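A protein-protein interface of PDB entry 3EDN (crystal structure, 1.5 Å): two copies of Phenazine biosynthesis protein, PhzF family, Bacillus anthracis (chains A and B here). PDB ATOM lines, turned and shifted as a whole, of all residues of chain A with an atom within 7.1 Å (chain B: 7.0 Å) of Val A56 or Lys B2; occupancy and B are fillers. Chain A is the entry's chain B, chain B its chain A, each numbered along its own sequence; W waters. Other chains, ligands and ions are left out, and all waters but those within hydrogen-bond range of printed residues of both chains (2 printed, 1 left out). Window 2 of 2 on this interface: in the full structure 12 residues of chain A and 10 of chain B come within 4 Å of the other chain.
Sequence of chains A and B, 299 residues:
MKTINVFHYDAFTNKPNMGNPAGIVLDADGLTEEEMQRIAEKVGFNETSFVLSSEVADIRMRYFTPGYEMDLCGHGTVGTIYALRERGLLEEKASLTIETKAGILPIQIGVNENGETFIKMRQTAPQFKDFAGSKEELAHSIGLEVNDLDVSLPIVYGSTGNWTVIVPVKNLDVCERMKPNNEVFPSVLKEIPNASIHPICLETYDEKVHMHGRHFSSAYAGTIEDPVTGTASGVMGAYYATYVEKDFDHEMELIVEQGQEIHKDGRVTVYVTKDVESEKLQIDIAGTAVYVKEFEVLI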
ATOM      1  N   SER A  53     -20.668   6.058 -20.519  1.00  0.00           N
ATOM      2  CA  SER A  53     -21.183   4.787 -20.025  1.00  0.00           C
ATOM      3  C   SER A  53     -20.329   3.630 -20.527  1.00  0.00           C
ATOM      4  O   SER A  53     -19.718   3.712 -21.596  1.00  0.00           O
ATOM      5  CB  SER A  53     -22.619   4.574 -20.502  1.00  0.00           C
ATOM      6  OG  SER A  53     -23.496   5.437 -19.803  1.00  0.00           O
ATOM      7  N   SER A  54     -20.264   2.562 -19.730  1.00  0.00           N
ATOM      8  CA  SER A  54     -19.563   1.349 -20.106  1.00  0.00           C
ATOM      9  C   SER A  54     -20.401   0.138 -19.746  1.00  0.00           C
ATOM     10  O   SER A  54     -21.046   0.127 -18.691  1.00  0.00           O
ATOM     11  CB  SER A  54     -18.224   1.270 -19.375  1.00  0.00           C
ATOM     12  OG  SER A  54     -17.590   0.031 -19.648  1.00  0.00           O
ATOM     13  N   GLU A  55     -20.377  -0.862 -20.625  1.00  0.00           N
ATOM     14  CA  GLU A  55     -21.040  -2.139 -20.367  1.00  0.00           C
ATOM     15  C   GLU A  55     -20.094  -3.147 -19.709  1.00  0.00           C
ATOM     16  O   GLU A  55     -20.536  -4.217 -19.303  1.00  0.00           O
ATOM     17  CB  GLU A  55     -21.563  -2.767 -21.669  1.00  0.00           C
ATOM     18  CG  GLU A  55     -22.527  -1.908 -22.514  1.00  0.00           C
ATOM     19  CD  GLU A  55     -23.722  -1.367 -21.746  1.00  0.00           C
ATOM     20  OE1 GLU A  55     -24.109  -1.955 -20.712  1.00  0.00           O
ATOM     21  OE2 GLU A  55     -24.285  -0.347 -22.193  1.00  0.00           O
ATOM     22  N   VAL A  56     -18.803  -2.832 -19.612  1.00  0.00           N
ATOM     23  CA  VAL A  56     -17.834  -3.829 -19.150  1.00  0.00           C
ATOM     24  C   VAL A  56     -16.946  -3.341 -18.001  1.00  0.00           C
ATOM     25  O   VAL A  56     -16.099  -4.082 -17.518  1.00  0.00           O
ATOM     26  CB  VAL A  56     -16.925  -4.320 -20.308  1.00  0.00           C
ATOM     27  CG1 VAL A  56     -17.766  -4.998 -21.412  1.00  0.00           C
ATOM     28  CG2 VAL A  56     -16.104  -3.173 -20.877  1.00  0.00           C
ATOM     29  N   ALA A  57     -17.158  -2.109 -17.571  1.00  0.00           N
ATOM     30  CA  ALA A  57     -16.372  -1.499 -16.489  1.00  0.00           C
ATOM     31  C   ALA A  57     -17.240  -0.487 -15.765  1.00  0.00           C
ATOM     32  O   ALA A  57     -18.341  -0.180 -16.212  1.00  0.00           O
ATOM     33  CB  ALA A  57     -15.108  -0.817 -17.053  1.00  0.00           C
ATOM     34  N   ASP A  58     -16.743   0.075 -14.670  1.00  0.00           N
ATOM     35  CA  ASP A  58     -17.557   1.021 -13.923  1.00  0.00           C
ATOM     36  C   ASP A  58     -17.915   2.253 -14.750  1.00  0.00           C
ATOM     37  O   ASP A  58     -19.048   2.719 -14.729  1.00  0.00           O
ATOM     38  CB  ASP A  58     -16.857   1.412 -12.617  1.00  0.00           C
ATOM     39  CG  ASP A  58     -16.755   0.236 -11.663  1.00  0.00           C
ATOM     40  OD1 ASP A  58     -17.786  -0.419 -11.417  1.00  0.00           O
ATOM     41  OD2 ASP A  58     -15.644  -0.076 -11.208  1.00  0.00           O
ATOM     42  N   ILE A  59     -16.917   2.802 -15.446  1.00  0.00           N
ATOM     43  CA  ILE A  59     -17.125   3.944 -16.344  1.00  0.00           C
ATOM     44  C   ILE A  59     -16.245   3.734 -17.567  1.00  0.00           C
ATOM     45  O   ILE A  59     -15.424   2.814 -17.601  1.00  0.00           O
ATOM     46  CB  ILE A  59     -16.758   5.299 -15.707  1.00  0.00           C
ATOM     47  CG1 ILE A  59     -15.261   5.350 -15.401  1.00  0.00           C
ATOM     48  CG2 ILE A  59     -17.631   5.605 -14.466  1.00  0.00           C
ATOM     49  CD1 ILE A  59     -14.760   6.736 -14.986  1.00  0.00           C
ATOM     50  N   ARG A  60     -16.451   4.569 -18.580  1.00  0.00           N
ATOM     51  CA  ARG A  60     -15.612   4.611 -19.758  1.00  0.00           C
ATOM     52  C   ARG A  60     -15.058   6.027 -19.889  1.00  0.00           C
ATOM     53  O   ARG A  60     -15.702   6.994 -19.473  1.00  0.00           O
ATOM     54  CB  ARG A  60     -16.443   4.210 -20.978  1.00  0.00           C
ATOM     55  CG  ARG A  60     -15.685   4.230 -22.304  1.00  0.00           C
ATOM     56  CD  ARG A  60     -16.476   3.484 -23.381  1.00  0.00           C
ATOM     57  NE  ARG A  60     -17.766   4.124 -23.682  1.00  0.00           N
ATOM     58  CZ  ARG A  60     -17.967   4.997 -24.667  1.00  0.00           C
ATOM     59  NH1 ARG A  60     -16.963   5.362 -25.453  1.00  0.00           N
ATOM     60  NH2 ARG A  60     -19.173   5.518 -24.862  1.00  0.00           N
ATOM     61  N   THR A  97     -12.939   0.098 -12.185  1.00  0.00           N
ATOM     62  CA  THR A  97     -12.358  -0.133 -13.495  1.00  0.00           C
ATOM     63  C   THR A  97     -12.852   0.933 -14.456  1.00  0.00           C
ATOM     64  O   THR A  97     -13.983   1.408 -14.341  1.00  0.00           O
ATOM     65  CB  THR A  97     -12.706  -1.529 -14.040  1.00  0.00           C
ATOM     66  OG1 THR A  97     -14.123  -1.720 -14.017  1.00  0.00           O
ATOM     67  CG2 THR A  97     -12.026  -2.622 -13.197  1.00  0.00           C
ATOM     68  N   ILE A  98     -11.978   1.308 -15.390  1.00  0.00           N
ATOM     69  CA  ILE A  98     -12.279   2.303 -16.410  1.00  0.00           C
ATOM     70  C   ILE A  98     -12.048   1.695 -17.779  1.00  0.00           C
ATOM     71  O   ILE A  98     -10.949   1.262 -18.092  1.00  0.00           O
ATOM     72  CB  ILE A  98     -11.341   3.524 -16.323  1.00  0.00           C
ATOM     73  CG1 ILE A  98     -11.453   4.221 -14.963  1.00  0.00           C
ATOM     74  CG2 ILE A  98     -11.664   4.498 -17.437  1.00  0.00           C
ATOM     75  CD1 ILE A  98     -10.374   5.285 -14.779  1.00  0.00           C
ATOM     76  N   GLU A  99     -13.080   1.675 -18.610  1.00  0.00           N
ATOM     77  CA  GLU A  99     -12.906   1.240 -19.981  1.00  0.00           C
ATOM     78  C   GLU A  99     -12.319   2.368 -20.815  1.00  0.00           C
ATOM     79  O   GLU A  99     -12.827   3.493 -20.809  1.00  0.00           O
ATOM     80  CB  GLU A  99     -14.250   0.793 -20.576  1.00  0.00           C
ATOM     81  CG  GLU A  99     -14.112   0.264 -21.999  1.00  0.00           C
ATOM     82  CD  GLU A  99     -15.434  -0.117 -22.646  1.00  0.00           C
ATOM     83  OE1 GLU A  99     -16.510   0.207 -22.105  1.00  0.00           O
ATOM     84  OE2 GLU A  99     -15.380  -0.769 -23.715  1.00  0.00           O
ATOM     85  N   ILE A 104      -9.043  -1.963 -20.379  1.00  0.00           N
ATOM     86  CA  ILE A 104      -9.692  -1.680 -19.104  1.00  0.00           C
ATOM     87  C   ILE A 104      -8.626  -1.430 -18.047  1.00  0.00           C
ATOM     88  O   ILE A 104      -7.744  -2.265 -17.841  1.00  0.00           O
ATOM     89  CB  ILE A 104     -10.658  -2.819 -18.688  1.00  0.00           C
ATOM     90  CG1 ILE A 104     -11.814  -2.945 -19.700  1.00  0.00           C
ATOM     91  CG2 ILE A 104     -11.207  -2.566 -17.297  1.00  0.00           C
ATOM     92  CD1 ILE A 104     -12.683  -4.214 -19.502  1.00  0.00           C
ATOM     93  N   MET B   1     -12.753  -9.351 -26.043  1.00  0.00           N
ATOM     94  CA  MET B   1     -13.981  -9.151 -26.874  1.00  0.00           C
ATOM     95  C   MET B   1     -15.167  -8.749 -26.014  1.00  0.00           C
ATOM     96  O   MET B   1     -15.287  -9.177 -24.865  1.00  0.00           O
ATOM     97  CB  MET B   1     -14.332 -10.422 -27.656  1.00  0.00           C
ATOM     98  CG  MET B   1     -13.237 -10.929 -28.584  1.00  0.00           C
ATOM     99  SD  MET B   1     -12.577  -9.574 -29.806  1.00  0.00           S
ATOM    100  CE  MET B   1     -14.184  -9.355 -30.881  1.00  0.00           C
ATOM    101  N   LYS B   2     -16.049  -7.930 -26.577  1.00  0.00           N
ATOM    102  CA  LYS B   2     -17.276  -7.553 -25.897  1.00  0.00           C
ATOM    103  C   LYS B   2     -18.452  -8.173 -26.633  1.00  0.00           C
ATOM    104  O   LYS B   2     -18.381  -8.399 -27.841  1.00  0.00           O
ATOM    105  CB  LYS B   2     -17.420  -6.035 -25.849  1.00  0.00           C
ATOM    106  CG  LYS B   2     -16.407  -5.357 -24.938  1.00  0.00           C
ATOM    107  CD  LYS B   2     -16.736  -3.886 -24.719  1.00  0.00           C
ATOM    108  CE  LYS B   2     -16.511  -3.067 -25.984  1.00  0.00           C
ATOM    109  NZ  LYS B   2     -16.998  -1.671 -25.803  1.00  0.00           N
ATOM    110  N   THR B   3     -19.526  -8.449 -25.902  1.00  0.00           N
ATOM    111  CA  THR B   3     -20.723  -9.037 -26.496  1.00  0.00           C
ATOM    112  C   THR B   3     -21.828  -8.002 -26.588  1.00  0.00           C
ATOM    113  O   THR B   3     -22.247  -7.438 -25.578  1.00  0.00           O
ATOM    114  CB  THR B   3     -21.222 -10.248 -25.696  1.00  0.00           C
ATOM    115  OG1 THR B   3     -20.229 -11.281 -25.722  1.00  0.00           O
ATOM    116  CG2 THR B   3     -22.522 -10.785 -26.308  1.00  0.00           C
ATOM    117  N   ILE B   4     -22.309  -7.768 -27.808  1.00  0.00           N
ATOM    118  CA  ILE B   4     -23.356  -6.773 -28.035  1.00  0.00           C
ATOM    119  C   ILE B   4     -24.617  -7.472 -28.517  1.00  0.00           C
ATOM    120  O   ILE B   4     -24.569  -8.234 -29.479  1.00  0.00           O
ATOM    121  CB  ILE B   4     -22.935  -5.746 -29.109  1.00  0.00           C
ATOM    122  CG1 ILE B   4     -21.523  -5.209 -28.853  1.00  0.00           C
ATOM    123  CG2 ILE B   4     -23.966  -4.614 -29.204  1.00  0.00           C
ATOM    124  CD1 ILE B   4     -21.315  -4.655 -27.473  1.00  0.00           C
ATOM    125  N   GLY B  30     -22.673   2.804 -24.473  1.00  0.00           N
ATOM    126  CA  GLY B  30     -21.366   2.209 -24.158  1.00  0.00           C
ATOM    127  C   GLY B  30     -20.402   2.027 -25.319  1.00  0.00           C
ATOM    128  O   GLY B  30     -19.358   1.384 -25.157  1.00  0.00           O
ATOM    129  N   LEU B  31     -20.735   2.602 -26.477  1.00  0.00           N
ATOM    130  CA  LEU B  31     -20.007   2.330 -27.725  1.00  0.00           C
ATOM    131  C   LEU B  31     -19.403   3.580 -28.349  1.00  0.00           C
ATOM    132  O   LEU B  31     -19.986   4.656 -28.307  1.00  0.00           O
ATOM    133  CB  LEU B  31     -20.962   1.725 -28.759  1.00  0.00           C
ATOM    134  CG  LEU B  31     -21.567   0.390 -28.333  1.00  0.00           C
ATOM    135  CD1 LEU B  31     -22.699   0.001 -29.240  1.00  0.00           C
ATOM    136  CD2 LEU B  31     -20.476  -0.679 -28.325  1.00  0.00           C
ATOM    137  N   THR B  32     -18.229   3.428 -28.956  1.00  0.00           N
ATOM    138  CA  THR B  32     -17.668   4.480 -29.790  1.00  0.00           C
ATOM    139  C   THR B  32     -18.245   4.401 -31.203  1.00  0.00           C
ATOM    140  O   THR B  32     -18.808   3.375 -31.602  1.00  0.00           O
ATOM    141  CB  THR B  32     -16.156   4.333 -29.936  1.00  0.00           C
ATOM    142  OG1 THR B  32     -15.863   3.141 -30.692  1.00  0.00           O
ATOM    143  CG2 THR B  32     -15.491   4.232 -28.549  1.00  0.00           C
ATOM    144  N   GLU B  35     -16.797   1.461 -33.045  1.00  0.00           N
ATOM    145  CA  GLU B  35     -17.501   0.251 -32.675  1.00  0.00           C
ATOM    146  C   GLU B  35     -18.857   0.166 -33.364  1.00  0.00           C
ATOM    147  O   GLU B  35     -19.249  -0.903 -33.825  1.00  0.00           O
ATOM    148  CB  GLU B  35     -17.658   0.176 -31.164  1.00  0.00           C
ATOM    149  CG  GLU B  35     -16.334  -0.108 -30.468  1.00  0.00           C
ATOM    150  CD  GLU B  35     -16.437  -0.072 -28.960  1.00  0.00           C
ATOM    151  OE1 GLU B  35     -17.166   0.789 -28.414  1.00  0.00           O
ATOM    152  OE2 GLU B  35     -15.758  -0.903 -28.320  1.00  0.00           O
ATOM    153  N   VAL B 297     -23.248 -10.009 -31.323  1.00  0.00           N
ATOM    154  CA  VAL B 297     -22.109  -9.650 -32.153  1.00  0.00           C
ATOM    155  C   VAL B 297     -20.925  -9.394 -31.229  1.00  0.00           C
ATOM    156  O   VAL B 297     -21.078  -8.751 -30.199  1.00  0.00           O
ATOM    157  CB  VAL B 297     -22.417  -8.382 -32.978  1.00  0.00           C
ATOM    158  CG1 VAL B 297     -21.223  -7.971 -33.812  1.00  0.00           C
ATOM    159  CG2 VAL B 297     -23.640  -8.622 -33.877  1.00  0.00           C
ATOM    160  N   LEU B 298     -19.746  -9.899 -31.598  1.00  0.00           N
ATOM    161  CA  LEU B 298     -18.554  -9.678 -30.785  1.00  0.00           C
ATOM    162  C   LEU B 298     -17.676  -8.604 -31.405  1.00  0.00           C
ATOM    163  O   LEU B 298     -17.417  -8.625 -32.608  1.00  0.00           O
ATOM    164  CB  LEU B 298     -17.769 -10.980 -30.644  1.00  0.00           C
ATOM    165  CG  LEU B 298     -18.614 -12.156 -30.148  1.00  0.00           C
ATOM    166  CD1 LEU B 298     -17.914 -13.495 -30.407  1.00  0.00           C
ATOM    167  CD2 LEU B 298     -18.969 -12.000 -28.675  1.00  0.00           C
ATOM    168  N   ILE B 299     -17.227  -7.658 -30.583  1.00  0.00           N
ATOM    169  CA  ILE B 299     -16.350  -6.595 -31.063  1.00  0.00           C
ATOM    170  C   ILE B 299     -15.248  -6.245 -30.071  1.00  0.00           C
ATOM    171  O   ILE B 299     -15.181  -6.791 -28.968  1.00  0.00           O
ATOM    172  CB  ILE B 299     -17.124  -5.309 -31.362  1.00  0.00           C
ATOM    173  CG1 ILE B 299     -17.837  -4.828 -30.093  1.00  0.00           C
ATOM    174  CG2 ILE B 299     -18.079  -5.526 -32.544  1.00  0.00           C
ATOM    175  CD1 ILE B 299     -18.169  -3.374 -30.088  1.00  0.00           C
ATOM    176  OXT ILE B 299     -14.429  -5.370 -30.374  1.00  0.00           O
HETATM  177  O   HOH W   1     -24.021   0.298 -24.925  1.00  0.00           O
HETATM  178  O   HOH W   2     -18.927  -0.280 -23.121  1.00  0.00           O
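The side-chain amino group (NZ) of Lys B2 lies within salt-bridge range of the side-chain carboxylate (OE2) of Glu A99 (2.8 Å). NE of Arg A60 is in hydrogen-bond range of O of Gly B30, 3.5 Å away.
The side-chain amino group (NZ) of Lys B2 is in salt-bridge range of the side-chain carboxylate (OE2) of Glu B35. O of Ile B299 sits at hydrogen-bond distance from N of Lys B2, 2.8 Å away. N of Thr B32 sits at hydrogen-bond distance from OE1 of Glu B35, 2.9 Å away. O of Ser A53 sits at hydrogen-bond distance from NE of Arg A60 (2.9 Å). The side-chain hydroxyl of Ser A54 sits at hydrogen-bond distance from the backbone NH of Val A56, 3.1 Å away. The side-chain carboxylate of Glu A99 is in hydrogen-bond range of the side-chain hydroxyl of Ser A54 (2.7 Å).
Among the printed residues, pairs that only touch across the chains: Ser A53 with Gly B30, Arg A60 with Thr B32, Val A56 with Lys B2 and Arg A60 with Leu B31.
Ser A54 touches none of the printed residues of chain B. Of chain B, only Lys B2 comes within 4 Å of Val A56. Printed residues of chain B within 4 Å of Glu A99: Lys B2. Lys B2 touches just these residues of chain A: Val A56 and Glu A99. Of the printed residues of chain A, Gly B30 touches Ser A53 and Arg A60. Ile B299 touches none of the printed residues of chain A. The nearest residue of chain B that does not touch Val A56 is Thr B3 (5.9 Å). The nearest residue of chain A that does not touch Lys B2 is Arg A60 (5.7 Å). The nearest printed residue of chain B that does not touch Glu A99 is Gly B30 (4.3 Å).
Of the 11 printed residues of chain B, 4 touch a printed residue of chain A. Along chain B the printed residues that touch a printed residue of chain A span positions 2 to 32. Hydrophobic or aromatic side chains of chain A that line the printed part of chain B: Val A56. Among the printed residues, Asp or Glu carboxylates within 4 Å of a Lys or Arg side-chain nitrogen of the other chain: Glu A99 with Lys B2 (2.8 Å).
No position is printed for both chains. Of the 6 pairs that touch across the chains among the printed residues, none has its exchanged pair printed and touching as well.
Water W2 lies within hydrogen-bond range of O of Gly B30, OE1 of Glu A99 and N of Glu A55. Water W1 bridges the side-chain carboxylate of Glu A55 (2.8 Å) and the backbone NH of Gly B30 (2.9 Å).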
